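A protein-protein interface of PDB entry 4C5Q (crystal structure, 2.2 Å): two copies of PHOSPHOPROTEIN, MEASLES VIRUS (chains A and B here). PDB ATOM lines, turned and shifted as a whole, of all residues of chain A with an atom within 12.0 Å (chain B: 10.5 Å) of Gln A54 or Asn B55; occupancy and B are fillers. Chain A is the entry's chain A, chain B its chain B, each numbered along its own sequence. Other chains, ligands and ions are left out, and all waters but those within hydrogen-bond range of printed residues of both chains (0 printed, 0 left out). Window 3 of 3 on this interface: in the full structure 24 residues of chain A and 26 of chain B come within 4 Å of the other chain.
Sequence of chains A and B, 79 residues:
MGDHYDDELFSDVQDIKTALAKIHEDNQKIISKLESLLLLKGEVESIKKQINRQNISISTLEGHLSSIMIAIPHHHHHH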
ATOM      1  N   GLU A  43      -8.777  24.494  -1.557  1.00  0.00           N
ATOM      2  CA  GLU A  43      -9.791  23.498  -1.253  1.00  0.00           C
ATOM      3  C   GLU A  43     -10.594  23.171  -2.497  1.00  0.00           C
ATOM      4  O   GLU A  43     -10.753  21.997  -2.856  1.00  0.00           O
ATOM      5  CB  GLU A  43     -10.715  24.002  -0.153  1.00  0.00           C
ATOM      6  CG  GLU A  43      -9.990  24.322   1.141  1.00  0.00           C
ATOM      7  CD  GLU A  43      -9.121  23.170   1.597  1.00  0.00           C
ATOM      8  OE1 GLU A  43      -9.671  22.071   1.815  1.00  0.00           O
ATOM      9  OE2 GLU A  43      -7.887  23.353   1.720  1.00  0.00           O
ATOM     10  N   GLU A  45      -9.656  23.669  -5.521  1.00  0.00           N
ATOM     11  CA  GLU A  45      -8.719  22.913  -6.346  1.00  0.00           C
ATOM     12  C   GLU A  45      -8.630  21.440  -5.944  1.00  0.00           C
ATOM     13  O   GLU A  45      -8.549  20.584  -6.815  1.00  0.00           O
ATOM     14  CB  GLU A  45      -7.322  23.541  -6.340  1.00  0.00           C
ATOM     15  CG  GLU A  45      -7.141  24.714  -7.305  1.00  0.00           C
ATOM     16  CD  GLU A  45      -6.835  24.290  -8.732  1.00  0.00           C
ATOM     17  OE1 GLU A  45      -5.976  23.408  -8.934  1.00  0.00           O
ATOM     18  OE2 GLU A  45      -7.447  24.858  -9.660  1.00  0.00           O
ATOM     19  N   SER A  46      -8.650  21.138  -4.641  1.00  0.00           N
ATOM     20  CA  SER A  46      -8.573  19.744  -4.191  1.00  0.00           C
ATOM     21  C   SER A  46      -9.791  18.939  -4.622  1.00  0.00           C
ATOM     22  O   SER A  46      -9.665  17.809  -5.077  1.00  0.00           O
ATOM     23  CB  SER A  46      -8.449  19.645  -2.669  1.00  0.00           C
ATOM     24  OG  SER A  46      -7.269  20.250  -2.198  1.00  0.00           O
ATOM     25  N   ILE A  47     -10.971  19.523  -4.438  1.00  0.00           N
ATOM     26  CA  ILE A  47     -12.201  18.921  -4.927  1.00  0.00           C
ATOM     27  C   ILE A  47     -12.106  18.626  -6.424  1.00  0.00           C
ATOM     28  O   ILE A  47     -12.417  17.520  -6.862  1.00  0.00           O
ATOM     29  CB  ILE A  47     -13.406  19.815  -4.648  1.00  0.00           C
ATOM     30  CG1 ILE A  47     -13.608  19.960  -3.140  1.00  0.00           C
ATOM     31  CG2 ILE A  47     -14.651  19.244  -5.291  1.00  0.00           C
ATOM     32  CD1 ILE A  47     -14.638  21.000  -2.761  1.00  0.00           C
ATOM     33  N   LYS A  48     -11.671  19.606  -7.205  1.00  0.00           N
ATOM     34  CA  LYS A  48     -11.500  19.394  -8.644  1.00  0.00           C
ATOM     35  C   LYS A  48     -10.577  18.198  -8.901  1.00  0.00           C
ATOM     36  O   LYS A  48     -10.859  17.343  -9.732  1.00  0.00           O
ATOM     37  CB  LYS A  48     -10.962  20.664  -9.314  1.00  0.00           C
ATOM     38  CG  LYS A  48     -10.874  20.574 -10.828  1.00  0.00           C
ATOM     39  CD  LYS A  48     -10.627  21.945 -11.486  1.00  0.00           C
ATOM     40  CE  LYS A  48      -9.279  22.520 -11.102  1.00  0.00           C
ATOM     41  NZ  LYS A  48      -8.877  23.676 -11.952  1.00  0.00           N
ATOM     42  N   LYS A  49      -9.494  18.126  -8.141  1.00  0.00           N
ATOM     43  CA  LYS A  49      -8.538  17.037  -8.261  1.00  0.00           C
ATOM     44  C   LYS A  49      -9.171  15.692  -7.883  1.00  0.00           C
ATOM     45  O   LYS A  49      -8.947  14.673  -8.540  1.00  0.00           O
ATOM     46  CB  LYS A  49      -7.354  17.344  -7.350  1.00  0.00           C
ATOM     47  CG  LYS A  49      -6.183  16.397  -7.427  1.00  0.00           C
ATOM     48  CD  LYS A  49      -5.073  16.891  -6.497  1.00  0.00           C
ATOM     49  CE  LYS A  49      -3.746  16.191  -6.765  1.00  0.00           C
ATOM     50  NZ  LYS A  49      -3.612  14.887  -6.070  1.00  0.00           N
ATOM     51  N   GLN A  50      -9.954  15.686  -6.815  1.00  0.00           N
ATOM     52  CA  GLN A  50     -10.575  14.451  -6.364  1.00  0.00           C
ATOM     53  C   GLN A  50     -11.623  13.974  -7.340  1.00  0.00           C
ATOM     54  O   GLN A  50     -11.795  12.780  -7.554  1.00  0.00           O
ATOM     55  CB  GLN A  50     -11.219  14.664  -5.008  1.00  0.00           C
ATOM     56  CG  GLN A  50     -10.236  14.788  -3.891  1.00  0.00           C
ATOM     57  CD  GLN A  50     -10.900  14.605  -2.561  1.00  0.00           C
ATOM     58  OE1 GLN A  50     -11.914  15.242  -2.264  1.00  0.00           O
ATOM     59  NE2 GLN A  50     -10.352  13.711  -1.750  1.00  0.00           N
ATOM     60  N   ILE A  51     -12.337  14.920  -7.931  1.00  0.00           N
ATOM     61  CA  ILE A  51     -13.372  14.570  -8.883  1.00  0.00           C
ATOM     62  C   ILE A  51     -12.747  14.013 -10.156  1.00  0.00           C
ATOM     63  O   ILE A  51     -13.344  13.176 -10.826  1.00  0.00           O
ATOM     64  CB  ILE A  51     -14.305  15.749  -9.143  1.00  0.00           C
ATOM     65  CG1 ILE A  51     -15.073  16.054  -7.866  1.00  0.00           C
ATOM     66  CG2 ILE A  51     -15.299  15.438 -10.255  1.00  0.00           C
ATOM     67  CD1 ILE A  51     -16.122  17.095  -8.037  1.00  0.00           C
ATOM     68  N   ASN A  52     -11.529  14.446 -10.464  1.00  0.00           N
ATOM     69  CA  ASN A  52     -10.822  13.892 -11.608  1.00  0.00           C
ATOM     70  C   ASN A  52     -10.288  12.479 -11.372  1.00  0.00           C
ATOM     71  O   ASN A  52     -10.281  11.665 -12.289  1.00  0.00           O
ATOM     72  CB  ASN A  52      -9.721  14.838 -12.095  1.00  0.00           C
ATOM     73  CG  ASN A  52     -10.274  16.011 -12.904  1.00  0.00           C
ATOM     74  OD1 ASN A  52      -9.608  17.033 -13.085  1.00  0.00           O
ATOM     75  ND2 ASN A  52     -11.502  15.869 -13.380  1.00  0.00           N
ATOM     76  N   ARG A  53      -9.842  12.188 -10.152  1.00  0.00           N
ATOM     77  CA  ARG A  53      -9.442  10.828  -9.803  1.00  0.00           C
ATOM     78  C   ARG A  53     -10.674   9.930  -9.759  1.00  0.00           C
ATOM     79  O   ARG A  53     -10.637   8.775 -10.180  1.00  0.00           O
ATOM     80  CB  ARG A  53      -8.710  10.807  -8.459  1.00  0.00           C
ATOM     81  CG  ARG A  53      -7.234  11.176  -8.555  1.00  0.00           C
ATOM     82  CD  ARG A  53      -6.762  12.043  -7.386  1.00  0.00           C
ATOM     83  NE  ARG A  53      -5.312  12.246  -7.410  1.00  0.00           N
ATOM     84  CZ  ARG A  53      -4.475  11.777  -6.486  1.00  0.00           C
ATOM     85  NH1 ARG A  53      -4.950  11.091  -5.454  1.00  0.00           N
ATOM     86  NH2 ARG A  53      -3.169  11.998  -6.584  1.00  0.00           N
ATOM     87  N   GLN A  54     -11.773  10.482  -9.264  1.00  0.00           N
ATOM     88  CA  GLN A  54     -13.038   9.768  -9.187  1.00  0.00           C
ATOM     89  C   GLN A  54     -13.560   9.394 -10.568  1.00  0.00           C
ATOM     90  O   GLN A  54     -13.987   8.261 -10.791  1.00  0.00           O
ATOM     91  CB  GLN A  54     -14.060  10.628  -8.452  1.00  0.00           C
ATOM     92  CG  GLN A  54     -15.462  10.071  -8.423  1.00  0.00           C
ATOM     93  CD  GLN A  54     -16.237  10.559  -7.217  1.00  0.00           C
ATOM     94  OE1 GLN A  54     -15.653  10.876  -6.177  1.00  0.00           O
ATOM     95  NE2 GLN A  54     -17.559  10.614  -7.343  1.00  0.00           N
ATOM     96  N   ASN A  55     -13.527  10.348 -11.493  1.00  0.00           N
ATOM     97  CA  ASN A  55     -13.977  10.096 -12.857  1.00  0.00           C
ATOM     98  C   ASN A  55     -13.151   9.015 -13.543  1.00  0.00           C
ATOM     99  O   ASN A  55     -13.613   8.375 -14.489  1.00  0.00           O
ATOM    100  CB  ASN A  55     -13.994  11.382 -13.676  1.00  0.00           C
ATOM    101  CG  ASN A  55     -15.295  12.139 -13.527  1.00  0.00           C
ATOM    102  OD1 ASN A  55     -16.054  11.903 -12.586  1.00  0.00           O
ATOM    103  ND2 ASN A  55     -15.566  13.050 -14.457  1.00  0.00           N
ATOM    104  N   ILE A  56     -11.928   8.812 -13.068  1.00  0.00           N
ATOM    105  CA  ILE A  56     -11.220   7.588 -13.392  1.00  0.00           C
ATOM    106  C   ILE A  56     -11.911   6.462 -12.613  1.00  0.00           C
ATOM    107  O   ILE A  56     -11.508   6.061 -11.513  1.00  0.00           O
ATOM    108  CB  ILE A  56      -9.696   7.718 -13.159  1.00  0.00           C
ATOM    109  CG1 ILE A  56      -9.129   8.736 -14.149  1.00  0.00           C
ATOM    110  CG2 ILE A  56      -8.978   6.386 -13.369  1.00  0.00           C
ATOM    111  CD1 ILE A  56      -7.709   9.159 -13.872  1.00  0.00           C
ATOM    112  N   SER A  57     -13.015   6.009 -13.192  1.00  0.00           N
ATOM    113  CA  SER A  57     -13.809   4.923 -12.651  1.00  0.00           C
ATOM    114  C   SER A  57     -14.227   4.114 -13.863  1.00  0.00           C
ATOM    115  O   SER A  57     -15.354   4.235 -14.357  1.00  0.00           O
ATOM    116  CB  SER A  57     -15.041   5.462 -11.936  1.00  0.00           C
ATOM    117  OG  SER A  57     -15.977   5.974 -12.869  1.00  0.00           O
ATOM    118  N   ILE A  58     -13.290   3.309 -14.353  1.00  0.00           N
ATOM    119  CA  ILE A  58     -13.493   2.486 -15.541  1.00  0.00           C
ATOM    120  C   ILE A  58     -14.514   1.355 -15.376  1.00  0.00           C
ATOM    121  O   ILE A  58     -14.831   0.647 -16.334  1.00  0.00           O
ATOM    122  CB  ILE A  58     -12.150   2.077 -16.176  1.00  0.00           C
ATOM    123  CG1 ILE A  58     -11.031   2.106 -15.132  1.00  0.00           C
ATOM    124  CG2 ILE A  58     -11.814   2.993 -17.344  1.00  0.00           C
ATOM    125  CD1 ILE A  58     -11.118   0.985 -14.119  1.00  0.00           C
ATOM    126  N   SER A  59     -15.035   1.206 -14.162  1.00  0.00           N
ATOM    127  CA  SER A  59     -16.098   0.247 -13.894  1.00  0.00           C
ATOM    128  C   SER A  59     -17.032  -0.009 -15.073  1.00  0.00           C
ATOM    129  O   SER A  59     -17.202   0.851 -15.940  1.00  0.00           O
ATOM    130  CB  SER A  59     -16.905   0.604 -12.643  1.00  0.00           C
ATOM    131  OG  SER A  59     -16.201   0.266 -11.461  1.00  0.00           O
ATOM    132  N   ILE B  47     -18.376  19.049   1.151  1.00  0.00           N
ATOM    133  CA  ILE B  47     -18.243  18.504  -0.182  1.00  0.00           C
ATOM    134  C   ILE B  47     -16.998  17.641  -0.273  1.00  0.00           C
ATOM    135  O   ILE B  47     -17.062  16.476  -0.697  1.00  0.00           O
ATOM    136  CB  ILE B  47     -18.205  19.601  -1.250  1.00  0.00           C
ATOM    137  CG1 ILE B  47     -19.588  20.239  -1.405  1.00  0.00           C
ATOM    138  CG2 ILE B  47     -17.797  19.012  -2.581  1.00  0.00           C
ATOM    139  CD1 ILE B  47     -19.590  21.574  -2.150  1.00  0.00           C
ATOM    140  N   LYS B  48     -15.871  18.201   0.144  1.00  0.00           N
ATOM    141  CA  LYS B  48     -14.619  17.447   0.195  1.00  0.00           C
ATOM    142  C   LYS B  48     -14.785  16.111   0.923  1.00  0.00           C
ATOM    143  O   LYS B  48     -14.292  15.084   0.477  1.00  0.00           O
ATOM    144  CB  LYS B  48     -13.531  18.283   0.872  1.00  0.00           C
ATOM    145  CG  LYS B  48     -12.114  17.897   0.481  1.00  0.00           C
ATOM    146  CD  LYS B  48     -11.090  18.886   1.065  1.00  0.00           C
ATOM    147  CE  LYS B  48      -9.683  18.594   0.544  1.00  0.00           C
ATOM    148  NZ  LYS B  48      -8.655  19.556   1.052  1.00  0.00           N
ATOM    149  N   LYS B  49     -15.502  16.137   2.036  1.00  0.00           N
ATOM    150  CA  LYS B  49     -15.688  14.968   2.877  1.00  0.00           C
ATOM    151  C   LYS B  49     -16.610  13.957   2.210  1.00  0.00           C
ATOM    152  O   LYS B  49     -16.341  12.750   2.208  1.00  0.00           O
ATOM    153  CB  LYS B  49     -16.280  15.440   4.204  1.00  0.00           C
ATOM    154  CG  LYS B  49     -16.870  14.390   5.116  1.00  0.00           C
ATOM    155  CD  LYS B  49     -17.639  15.117   6.224  1.00  0.00           C
ATOM    156  CE  LYS B  49     -18.320  14.180   7.211  1.00  0.00           C
ATOM    157  NZ  LYS B  49     -17.357  13.459   8.080  1.00  0.00           N
ATOM    158  N   GLN B  50     -17.704  14.445   1.642  1.00  0.00           N
ATOM    159  CA  GLN B  50     -18.635  13.555   0.976  1.00  0.00           C
ATOM    160  C   GLN B  50     -18.035  12.981  -0.312  1.00  0.00           C
ATOM    161  O   GLN B  50     -18.461  11.929  -0.787  1.00  0.00           O
ATOM    162  CB  GLN B  50     -19.957  14.274   0.712  1.00  0.00           C
ATOM    163  CG  GLN B  50     -20.591  14.879   1.960  1.00  0.00           C
ATOM    164  CD  GLN B  50     -20.841  13.866   3.092  1.00  0.00           C
ATOM    165  OE1 GLN B  50     -20.928  12.650   2.865  1.00  0.00           O
ATOM    166  NE2 GLN B  50     -20.969  14.375   4.320  1.00  0.00           N
ATOM    167  N   ILE B  51     -17.036  13.658  -0.868  1.00  0.00           N
ATOM    168  CA  ILE B  51     -16.372  13.145  -2.062  1.00  0.00           C
ATOM    169  C   ILE B  51     -15.334  12.092  -1.691  1.00  0.00           C
ATOM    170  O   ILE B  51     -15.172  11.098  -2.399  1.00  0.00           O
ATOM    171  CB  ILE B  51     -15.747  14.264  -2.915  1.00  0.00           C
ATOM    172  CG1 ILE B  51     -16.840  15.068  -3.598  1.00  0.00           C
ATOM    173  CG2 ILE B  51     -14.870  13.689  -4.011  1.00  0.00           C
ATOM    174  CD1 ILE B  51     -16.300  16.182  -4.436  1.00  0.00           C
ATOM    175  N   ASN B  52     -14.646  12.294  -0.573  1.00  0.00           N
ATOM    176  CA  ASN B  52     -13.744  11.262  -0.071  1.00  0.00           C
ATOM    177  C   ASN B  52     -14.511  10.023   0.364  1.00  0.00           C
ATOM    178  O   ASN B  52     -14.005   8.908   0.276  1.00  0.00           O
ATOM    179  CB  ASN B  52     -12.880  11.782   1.080  1.00  0.00           C
ATOM    180  CG  ASN B  52     -11.590  12.424   0.594  1.00  0.00           C
ATOM    181  OD1 ASN B  52     -10.900  11.880  -0.272  1.00  0.00           O
ATOM    182  ND2 ASN B  52     -11.266  13.594   1.137  1.00  0.00           N
ATOM    183  N   ARG B  53     -15.728  10.233   0.850  1.00  0.00           N
ATOM    184  CA  ARG B  53     -16.603   9.139   1.227  1.00  0.00           C
ATOM    185  C   ARG B  53     -16.973   8.375  -0.040  1.00  0.00           C
ATOM    186  O   ARG B  53     -16.936   7.147  -0.064  1.00  0.00           O
ATOM    187  CB  ARG B  53     -17.851   9.687   1.916  1.00  0.00           C
ATOM    188  CG  ARG B  53     -18.782   8.640   2.515  1.00  0.00           C
ATOM    189  CD  ARG B  53     -19.688   9.257   3.581  1.00  0.00           C
ATOM    190  NE  ARG B  53     -18.940   9.651   4.777  1.00  0.00           N
ATOM    191  CZ  ARG B  53     -18.506  10.886   5.027  1.00  0.00           C
ATOM    192  NH1 ARG B  53     -18.747  11.870   4.171  1.00  0.00           N
ATOM    193  NH2 ARG B  53     -17.828  11.141   6.140  1.00  0.00           N
ATOM    194  N   GLN B  54     -17.307   9.116  -1.096  1.00  0.00           N
ATOM    195  CA  GLN B  54     -17.627   8.519  -2.387  1.00  0.00           C
ATOM    196  C   GLN B  54     -16.459   7.730  -2.945  1.00  0.00           C
ATOM    197  O   GLN B  54     -16.645   6.631  -3.457  1.00  0.00           O
ATOM    198  CB  GLN B  54     -18.040   9.579  -3.408  1.00  0.00           C
ATOM    199  CG  GLN B  54     -19.496   9.958  -3.352  1.00  0.00           C
ATOM    200  CD  GLN B  54     -19.901  10.877  -4.487  1.00  0.00           C
ATOM    201  OE1 GLN B  54     -19.155  11.064  -5.451  1.00  0.00           O
ATOM    202  NE2 GLN B  54     -21.086  11.464  -4.375  1.00  0.00           N
ATOM    203  N   ASN B  55     -15.258   8.296  -2.860  1.00  0.00           N
ATOM    204  CA  ASN B  55     -14.070   7.624  -3.374  1.00  0.00           C
ATOM    205  C   ASN B  55     -13.856   6.229  -2.788  1.00  0.00           C
ATOM    206  O   ASN B  55     -13.273   5.370  -3.445  1.00  0.00           O
ATOM    207  CB  ASN B  55     -12.816   8.491  -3.213  1.00  0.00           C
ATOM    208  CG  ASN B  55     -12.656   9.496  -4.340  1.00  0.00           C
ATOM    209  OD1 ASN B  55     -13.349   9.425  -5.357  1.00  0.00           O
ATOM    210  ND2 ASN B  55     -11.736  10.438  -4.166  1.00  0.00           N
ATOM    211  N   ILE B  56     -14.328   6.004  -1.563  1.00  0.00           N
ATOM    212  CA  ILE B  56     -14.382   4.654  -1.007  1.00  0.00           C
ATOM    213  C   ILE B  56     -15.602   3.957  -1.611  1.00  0.00           C
ATOM    214  O   ILE B  56     -16.524   3.549  -0.903  1.00  0.00           O
ATOM    215  CB  ILE B  56     -14.477   4.641   0.544  1.00  0.00           C
ATOM    216  CG1 ILE B  56     -13.541   5.673   1.172  1.00  0.00           C
ATOM    217  CG2 ILE B  56     -14.147   3.255   1.095  1.00  0.00           C
ATOM    218  CD1 ILE B  56     -13.645   5.732   2.693  1.00  0.00           C
ATOM    219  N   SER B  57     -15.606   3.837  -2.933  1.00  0.00           N
ATOM    220  CA  SER B  57     -16.738   3.274  -3.650  1.00  0.00           C
ATOM    221  C   SER B  57     -16.510   1.806  -3.931  1.00  0.00           C
ATOM    222  O   SER B  57     -17.442   1.094  -4.295  1.00  0.00           O
ATOM    223  CB  SER B  57     -16.942   4.003  -4.974  1.00  0.00           C
ATOM    224  OG  SER B  57     -15.752   3.989  -5.739  1.00  0.00           O
ATOM    225  N   ILE B  58     -15.267   1.366  -3.757  1.00  0.00           N
ATOM    226  CA  ILE B  58     -14.857   0.005  -4.108  1.00  0.00           C
ATOM    227  C   ILE B  58     -15.634  -1.097  -3.383  1.00  0.00           C
ATOM    228  O   ILE B  58     -16.043  -0.937  -2.231  1.00  0.00           O
ATOM    229  CB  ILE B  58     -13.346  -0.196  -3.878  1.00  0.00           C
ATOM    230  CG1 ILE B  58     -13.009  -0.158  -2.386  1.00  0.00           C
ATOM    231  CG2 ILE B  58     -12.553   0.863  -4.623  1.00  0.00           C
ATOM    232  CD1 ILE B  58     -12.643  -1.512  -1.811  1.00  0.00           C
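NE2 of Gln A54 lies within hydrogen-bond range of OE1 of Gln B54.
The side-chain amide nitrogen (NE2) of Gln A50 lies within hydrogen-bond range of the side-chain amide oxygen (OD1) of Asn B52, at 2.4 Å.
The side-chain amide oxygen (OD1) of Asn B55 lies close to the side-chain amide oxygen (OE1) of Gln A54 (2.8 Å).
The side-chain carboxylate of Glu A43 is in salt-bridge range of the side-chain amino group of Lys B48 (2.8 Å).
The side-chain amide oxygen (OD1) of Asn A55 lies close to the backbone carbonyl oxygen (O) of Ile A51, 3.5 Å away.
The backbone carbonyl oxygen (O) of Lys B48 is in hydrogen-bond range of the side-chain amide nitrogen (ND2) of Asn B52, 3.4 Å away.
Among the printed residues, pairs that only touch across the chains: Ile A47 with Ile B51, Ser A46 with Lys B48, Gln A50 with Lys B48, Gln A54 with Ile B51, Ile A51 with Ile B51, Ile A47 with Ile B47 and Gln A50 with Ile B51.
Of the printed residues of chain B, Glu A43 touches Lys B48 (2.8 Å).
Gln A50 touches just these residues of chain B: Lys B48 (3.6 Å), Ile B51 (3.8 Å) and Asn B52 (2.4 Å).
Printed residues of chain B within 4 Å of Ile A51: Ile B51 (3.6 Å).
Printed residues of chain B within 4 Å of Gln A54: Ile B51, Gln B54 and Asn B55.
No residue of chain B comes within 4 Å of Asn A55.
No residue of chain B comes within 4 Å of Ser A57.
Ile B51 touches four residues of chain A.
Gln B54 touches one residue of chain A.
Of chain A, only Gln A54 (2.8 Å) comes within 4 Å of Asn B55.
Ile B56 touches none of the printed residues of chain A.
Ile B58 touches none of the printed residues of chain A.
The nearest residue of chain B that does not touch Gln A54 is Asn B52 (5.9 Å).
Printed residues of chain B that touch a printed residue of chain A: Ile B47, Lys B48, Ile B51, Asn B52, Gln B54 and Asn B55.
Hydrophobic or aromatic side chains of chain A that line the printed part of chain B: Ile A47 and Ile A51.
Gln A50 touches Lys B48, but with the chains exchanged Lys A48 does not touch Gln B50 (11.5 Å).
Gln A50 touches Ile B51, but with the chains exchanged Ile A51 does not touch Gln B50 (8.7 Å).
Gln A50 touches Asn B52, but with the chains exchanged Asn A52 does not touch Gln B50 (12.1 Å).
Gln A54 touches its own counterpart, Gln B54.
Positions printed for both chains: 47, 48, 49, 50, 51, 52, 53, 54, 55, 56, 57 and 58.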
